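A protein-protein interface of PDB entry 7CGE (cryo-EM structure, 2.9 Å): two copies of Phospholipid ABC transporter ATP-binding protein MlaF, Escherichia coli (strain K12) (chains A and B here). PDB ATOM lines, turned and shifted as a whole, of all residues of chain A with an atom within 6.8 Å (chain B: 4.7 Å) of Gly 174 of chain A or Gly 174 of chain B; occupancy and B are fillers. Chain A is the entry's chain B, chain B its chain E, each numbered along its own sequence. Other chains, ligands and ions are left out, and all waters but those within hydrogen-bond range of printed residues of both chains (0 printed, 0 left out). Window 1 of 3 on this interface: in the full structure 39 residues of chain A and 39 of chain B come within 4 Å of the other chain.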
ATOM      1  N   SER A  43      16.370  22.361  -1.677  1.00  0.00           N
ATOM      2  CA  SER A  43      16.756  21.079  -2.247  1.00  0.00           C
ATOM      3  C   SER A  43      17.856  21.183  -3.289  1.00  0.00           C
ATOM      4  O   SER A  43      17.938  20.326  -4.172  1.00  0.00           O
ATOM      5  CB  SER A  43      15.544  20.390  -2.864  1.00  0.00           C
ATOM      6  OG  SER A  43      15.903  19.117  -3.361  1.00  0.00           O
ATOM      7  N   ARG A 151      17.200   1.114   4.211  1.00  0.00           N
ATOM      8  CA  ARG A 151      17.627   2.105   5.185  1.00  0.00           C
ATOM      9  C   ARG A 151      17.510   1.606   6.612  1.00  0.00           C
ATOM     10  O   ARG A 151      18.192   2.132   7.491  1.00  0.00           O
ATOM     11  CB  ARG A 151      16.813   3.382   5.033  1.00  0.00           C
ATOM     12  CG  ARG A 151      17.094   4.119   3.764  1.00  0.00           C
ATOM     13  CD  ARG A 151      16.294   5.383   3.678  1.00  0.00           C
ATOM     14  NE  ARG A 151      16.282   5.893   2.316  1.00  0.00           N
ATOM     15  CZ  ARG A 151      15.490   6.865   1.893  1.00  0.00           C
ATOM     16  NH1 ARG A 151      14.643   7.434   2.725  1.00  0.00           N
ATOM     17  NH2 ARG A 151      15.543   7.265   0.636  1.00  0.00           N
ATOM     18  N   PRO A 171      16.779  10.886   5.636  1.00  0.00           N
ATOM     19  CA  PRO A 171      16.147   9.593   5.913  1.00  0.00           C
ATOM     20  C   PRO A 171      14.770   9.476   5.312  1.00  0.00           C
ATOM     21  O   PRO A 171      14.372   8.381   4.903  1.00  0.00           O
ATOM     22  CB  PRO A 171      16.077   9.559   7.443  1.00  0.00           C
ATOM     23  CG  PRO A 171      16.877  10.680   7.897  1.00  0.00           C
ATOM     24  CD  PRO A 171      16.845  11.703   6.849  1.00  0.00           C
ATOM     25  N   PHE A 172      14.037  10.572   5.252  1.00  0.00           N
ATOM     26  CA  PHE A 172      12.669  10.611   4.771  1.00  0.00           C
ATOM     27  C   PHE A 172      12.745  11.297   3.423  1.00  0.00           C
ATOM     28  O   PHE A 172      12.732  12.526   3.364  1.00  0.00           O
ATOM     29  CB  PHE A 172      11.786  11.435   5.691  1.00  0.00           C
ATOM     30  CG  PHE A 172      12.093  11.278   7.130  1.00  0.00           C
ATOM     31  CD1 PHE A 172      11.722  10.146   7.817  1.00  0.00           C
ATOM     32  CD2 PHE A 172      12.724  12.301   7.818  1.00  0.00           C
ATOM     33  CE1 PHE A 172      12.007  10.029   9.149  1.00  0.00           C
ATOM     34  CE2 PHE A 172      12.999  12.185   9.149  1.00  0.00           C
ATOM     35  CZ  PHE A 172      12.643  11.051   9.816  1.00  0.00           C
ATOM     36  N   VAL A 173      12.869  10.533   2.347  1.00  0.00           N
ATOM     37  CA  VAL A 173      12.813  11.135   1.021  1.00  0.00           C
ATOM     38  C   VAL A 173      12.240  10.114   0.047  1.00  0.00           C
ATOM     39  O   VAL A 173      12.727   8.986  -0.069  1.00  0.00           O
ATOM     40  CB  VAL A 173      14.182  11.712   0.589  1.00  0.00           C
ATOM     41  CG1 VAL A 173      15.304  10.698   0.647  1.00  0.00           C
ATOM     42  CG2 VAL A 173      14.095  12.322  -0.775  1.00  0.00           C
ATOM     43  N   GLY A 174      11.151  10.490  -0.611  1.00  0.00           N
ATOM     44  CA  GLY A 174      10.431   9.566  -1.460  1.00  0.00           C
ATOM     45  C   GLY A 174       9.787   8.417  -0.726  1.00  0.00           C
ATOM     46  O   GLY A 174       9.582   7.358  -1.317  1.00  0.00           O
ATOM     47  N   GLN A 175       9.450   8.595   0.544  1.00  0.00           N
ATOM     48  CA  GLN A 175       8.969   7.496   1.359  1.00  0.00           C
ATOM     49  C   GLN A 175       7.487   7.637   1.665  1.00  0.00           C
ATOM     50  O   GLN A 175       6.940   8.736   1.743  1.00  0.00           O
ATOM     51  CB  GLN A 175       9.755   7.383   2.665  1.00  0.00           C
ATOM     52  CG  GLN A 175      11.154   6.823   2.509  1.00  0.00           C
ATOM     53  CD  GLN A 175      11.208   5.605   1.622  1.00  0.00           C
ATOM     54  OE1 GLN A 175      10.525   4.620   1.863  1.00  0.00           O
ATOM     55  NE2 GLN A 175      12.019   5.669   0.583  1.00  0.00           N
ATOM     56  N   ASP A 176       6.862   6.489   1.838  1.00  0.00           N
ATOM     57  CA  ASP A 176       5.455   6.363   2.159  1.00  0.00           C
ATOM     58  C   ASP A 176       5.203   6.839   3.593  1.00  0.00           C
ATOM     59  O   ASP A 176       6.128   6.868   4.403  1.00  0.00           O
ATOM     60  CB  ASP A 176       5.087   4.892   1.900  1.00  0.00           C
ATOM     61  CG  ASP A 176       3.745   4.464   2.422  1.00  0.00           C
ATOM     62  OD1 ASP A 176       3.503   4.408   3.633  1.00  0.00           O
ATOM     63  OD2 ASP A 176       2.868   4.233   1.590  1.00  0.00           O
ATOM     64  N   MET A 180       7.744   6.362   6.740  1.00  0.00           N
ATOM     65  CA  MET A 180       8.227   7.500   7.509  1.00  0.00           C
ATOM     66  C   MET A 180       7.870   7.367   8.979  1.00  0.00           C
ATOM     67  O   MET A 180       8.597   7.871   9.836  1.00  0.00           O
ATOM     68  CB  MET A 180       7.650   8.800   6.968  1.00  0.00           C
ATOM     69  CG  MET A 180       8.283   9.328   5.714  1.00  0.00           C
ATOM     70  SD  MET A 180       7.537  10.905   5.291  1.00  0.00           S
ATOM     71  CE  MET A 180       8.244  11.200   3.686  1.00  0.00           C
ATOM     72  N   HIS A 203      14.732  17.835   4.138  1.00  0.00           N
ATOM     73  CA  HIS A 203      13.797  18.896   3.782  1.00  0.00           C
ATOM     74  C   HIS A 203      12.360  18.421   3.919  1.00  0.00           C
ATOM     75  O   HIS A 203      11.485  18.874   3.188  1.00  0.00           O
ATOM     76  CB  HIS A 203      14.039  19.446   2.376  1.00  0.00           C
ATOM     77  CG  HIS A 203      14.047  18.416   1.290  1.00  0.00           C
ATOM     78  ND1 HIS A 203      15.142  18.210   0.483  1.00  0.00           N
ATOM     79  CD2 HIS A 203      13.095  17.558   0.853  1.00  0.00           C
ATOM     80  CE1 HIS A 203      14.869  17.264  -0.395  1.00  0.00           C
ATOM     81  NE2 HIS A 203      13.635  16.848  -0.188  1.00  0.00           N
ATOM     82  N   ASP A 204      12.099  17.494   4.828  1.00  0.00           N
ATOM     83  CA  ASP A 204      10.736  17.087   5.148  1.00  0.00           C
ATOM     84  C   ASP A 204      10.394  17.711   6.489  1.00  0.00           C
ATOM     85  O   ASP A 204      10.721  17.162   7.539  1.00  0.00           O
ATOM     86  CB  ASP A 204      10.589  15.575   5.196  1.00  0.00           C
ATOM     87  CG  ASP A 204      10.716  14.940   3.842  1.00  0.00           C
ATOM     88  OD1 ASP A 204      11.260  15.572   2.922  1.00  0.00           O
ATOM     89  OD2 ASP A 204      10.211  13.823   3.678  1.00  0.00           O
ATOM     90  N   PHE B 172       4.769  14.613  -6.758  1.00  0.00           N
ATOM     91  CA  PHE B 172       5.381  15.063  -5.522  1.00  0.00           C
ATOM     92  C   PHE B 172       6.113  13.851  -4.982  1.00  0.00           C
ATOM     93  O   PHE B 172       5.504  13.026  -4.303  1.00  0.00           O
ATOM     94  CB  PHE B 172       4.330  15.491  -4.513  1.00  0.00           C
ATOM     95  CG  PHE B 172       3.174  16.200  -5.103  1.00  0.00           C
ATOM     96  CD1 PHE B 172       3.277  17.505  -5.523  1.00  0.00           C
ATOM     97  CD2 PHE B 172       1.948  15.562  -5.198  1.00  0.00           C
ATOM     98  CE1 PHE B 172       2.190  18.143  -6.054  1.00  0.00           C
ATOM     99  CE2 PHE B 172       0.863  16.203  -5.722  1.00  0.00           C
ATOM    100  CZ  PHE B 172       0.983  17.492  -6.150  1.00  0.00           C
ATOM    101  N   VAL B 173       7.392  13.708  -5.304  1.00  0.00           N
ATOM    102  CA  VAL B 173       8.173  12.636  -4.704  1.00  0.00           C
ATOM    103  C   VAL B 173       9.625  13.087  -4.605  1.00  0.00           C
ATOM    104  O   VAL B 173      10.241  13.499  -5.591  1.00  0.00           O
ATOM    105  CB  VAL B 173       7.984  11.293  -5.450  1.00  0.00           C
ATOM    106  CG1 VAL B 173       8.288  11.384  -6.930  1.00  0.00           C
ATOM    107  CG2 VAL B 173       8.799  10.212  -4.813  1.00  0.00           C
ATOM    108  N   GLY B 174      10.155  13.073  -3.389  1.00  0.00           N
ATOM    109  CA  GLY B 174      11.474  13.608  -3.139  1.00  0.00           C
ATOM    110  C   GLY B 174      11.595  15.095  -3.350  1.00  0.00           C
ATOM    111  O   GLY B 174      12.687  15.579  -3.643  1.00  0.00           O
ATOM    112  N   GLN B 175      10.509  15.840  -3.200  1.00  0.00           N
ATOM    113  CA  GLN B 175      10.508  17.251  -3.533  1.00  0.00           C
ATOM    114  C   GLN B 175      10.434  18.118  -2.287  1.00  0.00           C
ATOM    115  O   GLN B 175       9.875  17.735  -1.260  1.00  0.00           O
ATOM    116  CB  GLN B 175       9.355  17.602  -4.471  1.00  0.00           C
ATOM    117  CG  GLN B 175       9.543  17.135  -5.901  1.00  0.00           C
ATOM    118  CD  GLN B 175      10.920  17.425  -6.440  1.00  0.00           C
ATOM    119  OE1 GLN B 175      11.367  18.565  -6.445  1.00  0.00           O
ATOM    120  NE2 GLN B 175      11.606  16.393  -6.894  1.00  0.00           N
ATOM    121  N   ASP B 176      11.016  19.295  -2.414  1.00  0.00           N
ATOM    122  CA  ASP B 176      11.060  20.303  -1.374  1.00  0.00           C
ATOM    123  C   ASP B 176       9.663  20.895  -1.163  1.00  0.00           C
ATOM    124  O   ASP B 176       8.819  20.813  -2.054  1.00  0.00           O
ATOM    125  CB  ASP B 176      12.126  21.321  -1.813  1.00  0.00           C
ATOM    126  CG  ASP B 176      12.156  22.600  -1.023  1.00  0.00           C
ATOM    127  OD1 ASP B 176      11.226  23.415  -1.066  1.00  0.00           O
ATOM    128  OD2 ASP B 176      13.119  22.775  -0.276  1.00  0.00           O
ATOM    129  N   HIS B 203       1.673   8.904  -3.252  1.00  0.00           N
ATOM    130  CA  HIS B 203       1.557   8.522  -1.850  1.00  0.00           C
ATOM    131  C   HIS B 203       1.947   9.676  -0.940  1.00  0.00           C
ATOM    132  O   HIS B 203       2.458   9.458   0.154  1.00  0.00           O
ATOM    133  CB  HIS B 203       2.382   7.280  -1.508  1.00  0.00           C
ATOM    134  CG  HIS B 203       3.831   7.366  -1.876  1.00  0.00           C
ATOM    135  ND1 HIS B 203       4.420   6.481  -2.749  1.00  0.00           N
ATOM    136  CD2 HIS B 203       4.816   8.202  -1.471  1.00  0.00           C
ATOM    137  CE1 HIS B 203       5.700   6.775  -2.876  1.00  0.00           C
ATOM    138  NE2 HIS B 203       5.964   7.819  -2.115  1.00  0.00           N
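O of Val 173 of chain A sits at hydrogen-bond distance from NE2 of Gln 175 of chain A, at 3.5 Å.
The guanidinium group (NH2) of Arg 151 of chain A is in hydrogen-bond range of the backbone carbonyl oxygen (O) of Val 173 of chain A, at 3.4 Å.
NE2 of Gln 175 of chain B sits at hydrogen-bond distance from O of Val 173 of chain B.
Among the printed residues, pairs that only touch across the chains: Ser 43 of chain A with Asp 176 of chain B (3.6 Å), Gly 174 of chain A with His 203 of chain B (3.7 Å), Val 173 of chain A with Gly 174 of chain B (3.8 Å), Gly 174 of chain A with Val 173 of chain B (3.8 Å), His 203 of chain A with Gly 174 of chain B (3.8 Å), His 203 of chain A with Gln 175 of chain B (3.9 Å), Gln 175 of chain A with His 203 of chain B (3.9 Å) and Gly 174 of chain A with Gly 174 of chain B (3.9 Å).
Of chain B, only Val 173 (3.8 Å), Gly 174 (3.9 Å) and His 203 (3.7 Å) come within 4 Å of Gly 174 of chain A.
Gly 174 of chain B touches just these residues of chain A: Val 173 (3.8 Å), Gly 174 (3.9 Å) and His 203 (3.8 Å).
Printed residues of chain A within 4 Å of His 203 of chain B: Gly 174 (3.7 Å) and Gln 175 (3.9 Å).
Of the printed residues of chain B, Ser 43 of chain A touches Asp 176.
Printed residues of chain B within 4 Å of His 203 of chain A: Gly 174 (3.8 Å) and Gln 175 (3.9 Å).
Of the printed residues of chain B, Gln 175 of chain A touches His 203.
The nearest residue of chain A that does not touch Gly 174 of chain B is Ser 43 of chain A (4.8 Å).
Hydrophobic or aromatic side chains of chain B within 4 Å of the printed part of chain A: Val 173 and His 203.
Among the printed residues, no Asp or Glu carboxylate lies within 4 Å of a Lys or Arg side-chain nitrogen of the other chain.
Val 173 of chain A touches Gly 174 of chain B, and with the chains exchanged Gly 174 of chain A touches Val 173 of chain B.
Gly 174 of chain B touches its own counterpart, Gly 174 of chain A.
Gly 174 of chain A touches His 203 of chain B, and with the chains exchanged His 203 of chain A touches Gly 174 of chain B.
Gln 175 of chain A touches His 203 of chain B, and with the chains exchanged His 203 of chain A touches Gln 175 of chain B.
6 positions are printed for both chains.
Of the 8 pairs that touch across the chains among the printed residues, 7 have their exchanged pair printed and touching as well.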
